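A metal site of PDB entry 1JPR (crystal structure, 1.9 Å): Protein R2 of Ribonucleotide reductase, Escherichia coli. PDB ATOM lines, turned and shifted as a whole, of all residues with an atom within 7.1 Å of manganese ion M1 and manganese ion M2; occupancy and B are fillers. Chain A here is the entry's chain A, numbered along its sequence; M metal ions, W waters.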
ATOM      1  N   GLN A  80       4.688  -3.826  11.172  1.00  0.00           N
ATOM      2  CA  GLN A  80       5.392  -3.776   9.875  1.00  0.00           C
ATOM      3  C   GLN A  80       5.104  -5.097   9.108  1.00  0.00           C
ATOM      4  O   GLN A  80       4.812  -5.106   7.894  1.00  0.00           O
ATOM      5  CB  GLN A  80       6.893  -3.606  10.094  1.00  0.00           C
ATOM      6  CG  GLN A  80       7.205  -2.236  10.751  1.00  0.00           C
ATOM      7  CD  GLN A  80       8.691  -2.055  11.167  1.00  0.00           C
ATOM      8  OE1 GLN A  80       9.383  -3.017  11.569  1.00  0.00           O
ATOM      9  NE2 GLN A  80       9.179  -0.819  11.063  1.00  0.00           N
ATOM     10  N   LEU A  83       1.553  -5.032   7.722  1.00  0.00           N
ATOM     11  CA  LEU A  83       1.402  -4.166   6.546  1.00  0.00           C
ATOM     12  C   LEU A  83       2.022  -4.720   5.250  1.00  0.00           C
ATOM     13  O   LEU A  83       1.429  -4.623   4.161  1.00  0.00           O
ATOM     14  CB  LEU A  83       2.003  -2.773   6.845  1.00  0.00           C
ATOM     15  CG  LEU A  83       1.224  -1.898   7.870  1.00  0.00           C
ATOM     16  CD1 LEU A  83       1.852  -0.513   7.908  1.00  0.00           C
ATOM     17  CD2 LEU A  83      -0.232  -1.777   7.471  1.00  0.00           C
ATOM     18  N   ASP A  84       3.219  -5.306   5.361  1.00  0.00           N
ATOM     19  CA  ASP A  84       3.884  -5.786   4.161  1.00  0.00           C
ATOM     20  C   ASP A  84       3.248  -7.101   3.727  1.00  0.00           C
ATOM     21  O   ASP A  84       3.327  -7.419   2.542  1.00  0.00           O
ATOM     22  CB  ASP A  84       5.399  -5.913   4.353  1.00  0.00           C
ATOM     23  CG  ASP A  84       6.157  -4.574   4.074  1.00  0.00           C
ATOM     24  OD1 ASP A  84       6.001  -4.024   3.000  1.00  0.00           O
ATOM     25  OD2 ASP A  84       6.891  -4.044   4.901  1.00  0.00           O
ATOM     26  N   GLN A  87       0.584  -5.647   1.647  1.00  0.00           N
ATOM     27  CA  GLN A  87       1.132  -4.940   0.497  1.00  0.00           C
ATOM     28  C   GLN A  87       1.816  -5.852  -0.498  1.00  0.00           C
ATOM     29  O   GLN A  87       2.012  -5.462  -1.649  1.00  0.00           O
ATOM     30  CB  GLN A  87       2.113  -3.825   0.966  1.00  0.00           C
ATOM     31  CG  GLN A  87       1.264  -2.705   1.630  1.00  0.00           C
ATOM     32  CD  GLN A  87       0.383  -2.016   0.624  1.00  0.00           C
ATOM     33  OE1 GLN A  87       0.838  -1.208  -0.183  1.00  0.00           O
ATOM     34  NE2 GLN A  87      -0.880  -2.352   0.632  1.00  0.00           N
ATOM     35  N   TRP A 111       6.562  -3.296  -7.532  1.00  0.00           N
ATOM     36  CA  TRP A 111       6.306  -2.723  -6.211  1.00  0.00           C
ATOM     37  C   TRP A 111       5.820  -3.862  -5.303  1.00  0.00           C
ATOM     38  O   TRP A 111       6.358  -4.049  -4.195  1.00  0.00           O
ATOM     39  CB  TRP A 111       5.217  -1.675  -6.410  1.00  0.00           C
ATOM     40  CG  TRP A 111       4.487  -1.138  -5.202  1.00  0.00           C
ATOM     41  CD1 TRP A 111       4.874  -1.189  -3.884  1.00  0.00           C
ATOM     42  CD2 TRP A 111       3.255  -0.429  -5.247  1.00  0.00           C
ATOM     43  NE1 TRP A 111       3.914  -0.509  -3.092  1.00  0.00           N
ATOM     44  CE2 TRP A 111       2.913  -0.055  -3.919  1.00  0.00           C
ATOM     45  CE3 TRP A 111       2.363  -0.077  -6.285  1.00  0.00           C
ATOM     46  CZ2 TRP A 111       1.709   0.657  -3.624  1.00  0.00           C
ATOM     47  CZ3 TRP A 111       1.184   0.610  -5.977  1.00  0.00           C
ATOM     48  CH2 TRP A 111       0.865   0.963  -4.658  1.00  0.00           C
ATOM     49  N   SER A 114       8.598  -6.187  -4.388  1.00  0.00           N
ATOM     50  CA  SER A 114       9.537  -5.629  -3.419  1.00  0.00           C
ATOM     51  C   SER A 114       8.991  -5.731  -1.984  1.00  0.00           C
ATOM     52  O   SER A 114       9.762  -5.808  -1.036  1.00  0.00           O
ATOM     53  CB  SER A 114       9.921  -4.176  -3.818  1.00  0.00           C
ATOM     54  OG  SER A 114       8.846  -3.300  -3.529  1.00  0.00           O
ATOM     55  N   GLU A 115       7.657  -5.736  -1.824  1.00  0.00           N
ATOM     56  CA  GLU A 115       7.025  -5.899  -0.513  1.00  0.00           C
ATOM     57  C   GLU A 115       7.243  -7.339  -0.020  1.00  0.00           C
ATOM     58  O   GLU A 115       7.388  -7.586   1.195  1.00  0.00           O
ATOM     59  CB  GLU A 115       5.489  -5.574  -0.581  1.00  0.00           C
ATOM     60  CG  GLU A 115       5.108  -4.184  -1.143  1.00  0.00           C
ATOM     61  CD  GLU A 115       5.567  -3.001  -0.247  1.00  0.00           C
ATOM     62  OE1 GLU A 115       6.584  -3.155   0.451  1.00  0.00           O
ATOM     63  OE2 GLU A 115       4.959  -1.930  -0.295  1.00  0.00           O
ATOM     64  N   THR A 116       7.269  -8.305  -0.910  1.00  0.00           N
ATOM     65  CA  THR A 116       7.508  -9.698  -0.442  1.00  0.00           C
ATOM     66  C   THR A 116       8.919  -9.829   0.076  1.00  0.00           C
ATOM     67  O   THR A 116       9.185 -10.634   0.985  1.00  0.00           O
ATOM     68  CB  THR A 116       7.284 -10.815  -1.528  1.00  0.00           C
ATOM     69  OG1 THR A 116       8.253 -10.687  -2.582  1.00  0.00           O
ATOM     70  CG2 THR A 116       5.864 -10.725  -2.070  1.00  0.00           C
ATOM     71  N   HIS A 118      10.394  -7.384   1.663  1.00  0.00           N
ATOM     72  CA  HIS A 118      10.307  -6.833   3.041  1.00  0.00           C
ATOM     73  C   HIS A 118       9.782  -7.884   4.006  1.00  0.00           C
ATOM     74  O   HIS A 118      10.258  -8.045   5.175  1.00  0.00           O
ATOM     75  CB  HIS A 118       9.368  -5.634   3.006  1.00  0.00           C
ATOM     76  CG  HIS A 118       9.845  -4.525   2.143  1.00  0.00           C
ATOM     77  ND1 HIS A 118       9.136  -3.383   1.975  1.00  0.00           N
ATOM     78  CD2 HIS A 118      10.982  -4.359   1.432  1.00  0.00           C
ATOM     79  CE1 HIS A 118       9.801  -2.545   1.209  1.00  0.00           C
ATOM     80  NE2 HIS A 118      10.932  -3.118   0.867  1.00  0.00           N
ATOM     81  N   SER A 119       8.743  -8.619   3.571  1.00  0.00           N
ATOM     82  CA  SER A 119       8.202  -9.676   4.464  1.00  0.00           C
ATOM     83  C   SER A 119       9.274 -10.722   4.768  1.00  0.00           C
ATOM     84  O   SER A 119       9.361 -11.254   5.874  1.00  0.00           O
ATOM     85  CB  SER A 119       6.991 -10.430   3.797  1.00  0.00           C
ATOM     86  OG  SER A 119       5.944  -9.498   3.545  1.00  0.00           O
ATOM     87  N   TYR A 122      11.508  -9.554   7.505  1.00  0.00           N
ATOM     88  CA  TYR A 122      10.961  -9.650   8.896  1.00  0.00           C
ATOM     89  C   TYR A 122      11.096 -11.086   9.430  1.00  0.00           C
ATOM     90  O   TYR A 122      11.355 -11.313  10.647  1.00  0.00           O
ATOM     91  CB  TYR A 122       9.518  -9.211   8.961  1.00  0.00           C
ATOM     92  CG  TYR A 122       9.276  -7.847   8.389  1.00  0.00           C
ATOM     93  CD1 TYR A 122      10.101  -6.768   8.708  1.00  0.00           C
ATOM     94  CD2 TYR A 122       8.192  -7.618   7.538  1.00  0.00           C
ATOM     95  CE1 TYR A 122       9.865  -5.481   8.181  1.00  0.00           C
ATOM     96  CE2 TYR A 122       7.936  -6.358   7.012  1.00  0.00           C
ATOM     97  CZ  TYR A 122       8.768  -5.292   7.333  1.00  0.00           C
ATOM     98  OH  TYR A 122       8.466  -4.031   6.809  1.00  0.00           O
ATOM     99  N   VAL A 200      -3.764   3.786   0.180  1.00  0.00           N
ATOM    100  CA  VAL A 200      -2.457   3.181   0.084  1.00  0.00           C
ATOM    101  C   VAL A 200      -1.430   4.280   0.244  1.00  0.00           C
ATOM    102  O   VAL A 200      -0.345   4.071   0.835  1.00  0.00           O
ATOM    103  CB  VAL A 200      -2.243   2.498  -1.271  1.00  0.00           C
ATOM    104  CG1 VAL A 200      -0.815   1.963  -1.333  1.00  0.00           C
ATOM    105  CG2 VAL A 200      -3.278   1.377  -1.480  1.00  0.00           C
ATOM    106  N   LEU A 203      -0.960   4.725   3.840  1.00  0.00           N
ATOM    107  CA  LEU A 203      -0.343   3.608   4.460  1.00  0.00           C
ATOM    108  C   LEU A 203       1.197   3.697   4.292  1.00  0.00           C
ATOM    109  O   LEU A 203       1.950   3.547   5.247  1.00  0.00           O
ATOM    110  CB  LEU A 203      -0.858   2.322   3.785  1.00  0.00           C
ATOM    111  CG  LEU A 203      -0.388   0.959   4.326  1.00  0.00           C
ATOM    112  CD1 LEU A 203      -1.300  -0.124   3.697  1.00  0.00           C
ATOM    113  CD2 LEU A 203       1.129   0.669   3.878  1.00  0.00           C
ATOM    114  N   GLU A 204       1.649   3.953   3.085  1.00  0.00           N
ATOM    115  CA  GLU A 204       3.099   3.979   2.879  1.00  0.00           C
ATOM    116  C   GLU A 204       3.785   5.268   3.293  1.00  0.00           C
ATOM    117  O   GLU A 204       4.908   5.232   3.752  1.00  0.00           O
ATOM    118  CB  GLU A 204       3.397   3.655   1.425  1.00  0.00           C
ATOM    119  CG  GLU A 204       3.243   2.141   1.255  1.00  0.00           C
ATOM    120  CD  GLU A 204       3.378   1.715  -0.155  1.00  0.00           C
ATOM    121  OE1 GLU A 204       3.861   0.603  -0.367  1.00  0.00           O
ATOM    122  OE2 GLU A 204       2.972   2.502  -1.020  1.00  0.00           O
ATOM    123  N   PHE A 208       3.845   3.602   7.616  1.00  0.00           N
ATOM    124  CA  PHE A 208       5.169   2.978   7.639  1.00  0.00           C
ATOM    125  C   PHE A 208       6.223   3.884   8.220  1.00  0.00           C
ATOM    126  O   PHE A 208       7.154   3.388   8.842  1.00  0.00           O
ATOM    127  CB  PHE A 208       5.614   2.501   6.249  1.00  0.00           C
ATOM    128  CG  PHE A 208       5.506   1.005   6.089  1.00  0.00           C
ATOM    129  CD1 PHE A 208       6.289   0.178   6.886  1.00  0.00           C
ATOM    130  CD2 PHE A 208       4.570   0.452   5.235  1.00  0.00           C
ATOM    131  CE1 PHE A 208       6.134  -1.241   6.841  1.00  0.00           C
ATOM    132  CE2 PHE A 208       4.386  -0.954   5.170  1.00  0.00           C
ATOM    133  CZ  PHE A 208       5.178  -1.798   5.978  1.00  0.00           C
ATOM    134  N   PHE A 212       8.910   3.307  11.141  1.00  0.00           N
ATOM    135  CA  PHE A 212      10.363   3.453  10.963  1.00  0.00           C
ATOM    136  C   PHE A 212      10.943   4.238  12.129  1.00  0.00           C
ATOM    137  O   PHE A 212      12.010   3.903  12.618  1.00  0.00           O
ATOM    138  CB  PHE A 212      10.713   4.200   9.678  1.00  0.00           C
ATOM    139  CG  PHE A 212      10.255   3.531   8.440  1.00  0.00           C
ATOM    140  CD1 PHE A 212      10.096   2.183   8.393  1.00  0.00           C
ATOM    141  CD2 PHE A 212      10.009   4.299   7.266  1.00  0.00           C
ATOM    142  CE1 PHE A 212       9.678   1.545   7.162  1.00  0.00           C
ATOM    143  CE2 PHE A 212       9.597   3.669   6.064  1.00  0.00           C
ATOM    144  CZ  PHE A 212       9.437   2.300   6.040  1.00  0.00           C
ATOM    145  N   ILE A 234      14.410  -0.989   3.620  1.00  0.00           N
ATOM    146  CA  ILE A 234      12.938  -0.984   3.433  1.00  0.00           C
ATOM    147  C   ILE A 234      12.458   0.453   3.241  1.00  0.00           C
ATOM    148  O   ILE A 234      11.666   0.738   2.301  1.00  0.00           O
ATOM    149  CB  ILE A 234      12.235  -1.618   4.629  1.00  0.00           C
ATOM    150  CG1 ILE A 234      12.453  -3.139   4.587  1.00  0.00           C
ATOM    151  CG2 ILE A 234      10.695  -1.227   4.631  1.00  0.00           C
ATOM    152  CD1 ILE A 234      11.962  -3.893   5.800  1.00  0.00           C
ATOM    153  N   ASP A 237      12.960   1.738  -0.221  1.00  0.00           N
ATOM    154  CA  ASP A 237      11.962   1.203  -1.156  1.00  0.00           C
ATOM    155  C   ASP A 237      10.625   1.915  -0.918  1.00  0.00           C
ATOM    156  O   ASP A 237       9.947   2.284  -1.863  1.00  0.00           O
ATOM    157  CB  ASP A 237      11.705  -0.303  -0.930  1.00  0.00           C
ATOM    158  CG  ASP A 237      12.866  -1.166  -1.261  1.00  0.00           C
ATOM    159  OD1 ASP A 237      13.709  -0.758  -2.105  1.00  0.00           O
ATOM    160  OD2 ASP A 237      12.906  -2.301  -0.710  1.00  0.00           O
ATOM    161  N   GLU A 238      10.223   2.109   0.346  1.00  0.00           N
ATOM    162  CA  GLU A 238       8.958   2.793   0.580  1.00  0.00           C
ATOM    163  C   GLU A 238       8.926   4.212   0.003  1.00  0.00           C
ATOM    164  O   GLU A 238       7.843   4.678  -0.432  1.00  0.00           O
ATOM    165  CB  GLU A 238       8.631   2.847   2.100  1.00  0.00           C
ATOM    166  CG  GLU A 238       8.160   1.496   2.692  1.00  0.00           C
ATOM    167  CD  GLU A 238       7.166   0.720   1.758  1.00  0.00           C
ATOM    168  OE1 GLU A 238       6.189   1.376   1.254  1.00  0.00           O
ATOM    169  OE2 GLU A 238       7.377  -0.542   1.555  1.00  0.00           O
ATOM    170  N   ALA A 239      10.088   4.902   0.013  1.00  0.00           N
ATOM    171  CA  ALA A 239      10.142   6.267  -0.577  1.00  0.00           C
ATOM    172  C   ALA A 239       9.723   6.181  -2.061  1.00  0.00           C
ATOM    173  O   ALA A 239       9.026   7.056  -2.582  1.00  0.00           O
ATOM    174  CB  ALA A 239      11.570   6.855  -0.432  1.00  0.00           C
ATOM    175  N   HIS A 241       7.733   3.762  -3.386  1.00  0.00           N
ATOM    176  CA  HIS A 241       6.315   3.338  -3.414  1.00  0.00           C
ATOM    177  C   HIS A 241       5.397   4.521  -3.231  1.00  0.00           C
ATOM    178  O   HIS A 241       4.380   4.675  -3.929  1.00  0.00           O
ATOM    179  CB  HIS A 241       6.037   2.282  -2.342  1.00  0.00           C
ATOM    180  CG  HIS A 241       6.904   1.085  -2.494  1.00  0.00           C
ATOM    181  ND1 HIS A 241       6.948   0.059  -1.576  1.00  0.00           N
ATOM    182  CD2 HIS A 241       7.792   0.765  -3.460  1.00  0.00           C
ATOM    183  CE1 HIS A 241       7.831  -0.850  -1.976  1.00  0.00           C
ATOM    184  NE2 HIS A 241       8.357  -0.440  -3.128  1.00  0.00           N
ATOM    185  N   LEU A 242       5.754   5.382  -2.292  1.00  0.00           N
ATOM    186  CA  LEU A 242       4.883   6.536  -2.057  1.00  0.00           C
ATOM    187  C   LEU A 242       5.046   7.575  -3.154  1.00  0.00           C
ATOM    188  O   LEU A 242       4.113   8.360  -3.425  1.00  0.00           O
ATOM    189  CB  LEU A 242       5.126   7.085  -0.670  1.00  0.00           C
ATOM    190  CG  LEU A 242       6.425   7.804  -0.498  1.00  0.00           C
ATOM    191  CD1 LEU A 242       6.182   9.279  -0.862  1.00  0.00           C
ATOM    192  CD2 LEU A 242       6.860   7.693   0.976  1.00  0.00           C
HETATM  193 MN    MN M   1       7.179  -2.564   2.338  1.00  0.00          MN
HETATM  194 MN    MN M   2       5.671  -0.165   0.387  1.00  0.00          MN
HETATM  195  O   HOH W   1       7.439  -1.377   4.286  1.00  0.00           O
HETATM  196  O   HOH W   2       4.550  -0.615   2.352  1.00  0.00           O
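The side-chain carboxylate of Asp 84 lies within hydrogen-bond range of the side-chain hydroxyl of Tyr 122. O of Trp 111 is in hydrogen-bond range of OG of Ser 114 (2.7 Å). The backbone carbonyl oxygen (O) of Glu 115 is in hydrogen-bond range of the side-chain hydroxyl (OG) of Ser 119. A ring nitrogen (ND1) of His 241 sits close to the indole nitrogen (NE1) of Trp 111, at 3.4 Å. A ring nitrogen (NE2) of His 241 sits close to the backbone carbonyl oxygen of Asp 237 (3.4 Å). The side-chain hydroxyl (OG) of Ser 119 lies within hydrogen-bond range of the backbone carbonyl oxygen (O) of Asp 84, at 3.5 Å. The indole nitrogen (NE1) of Trp 111 lies close to the side-chain carboxylate (OE1) of Glu 204 (2.9 Å). The indole nitrogen of Trp 111 sits close to the side-chain carboxylate of Glu 115 (3.3 Å).
The nearest printed residue that does not touch manganese ion M1 is Phe 208 (4.2 Å).
Trp 111 touches manganese ion M2. Five residues have an atom within 4 Å of manganese ion M2: Trp 111, Glu 115, Glu 204, Glu 238 and His 241.
OD1 of Asp 84 binds manganese ion M1 (2.0 Å). The side-chain carboxylate (OE1) of Glu 115 binds manganese ion M1 (2.1 Å). ND1 of His 118 binds manganese ion M1, at 2.2 Å. OE2 of Glu 238 binds manganese ion M1. Water W1 is bound to manganese ion M1. Manganese ion M1 has five donor atoms within binding distance.
Manganese ion M2 is bound by the side-chain carboxylate (OE1) of Glu 238 (1.8 Å), the side-chain carboxylate (OE2) of Glu 115 (2.0 Å), the side-chain carboxylate (OE2) of Glu 238 (2.1 Å), the side-chain carboxylate (OE1) of Glu 204 (2.1 Å), water W2 (2.3 Å) and a ring nitrogen (ND1) of His 241 (2.4 Å).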
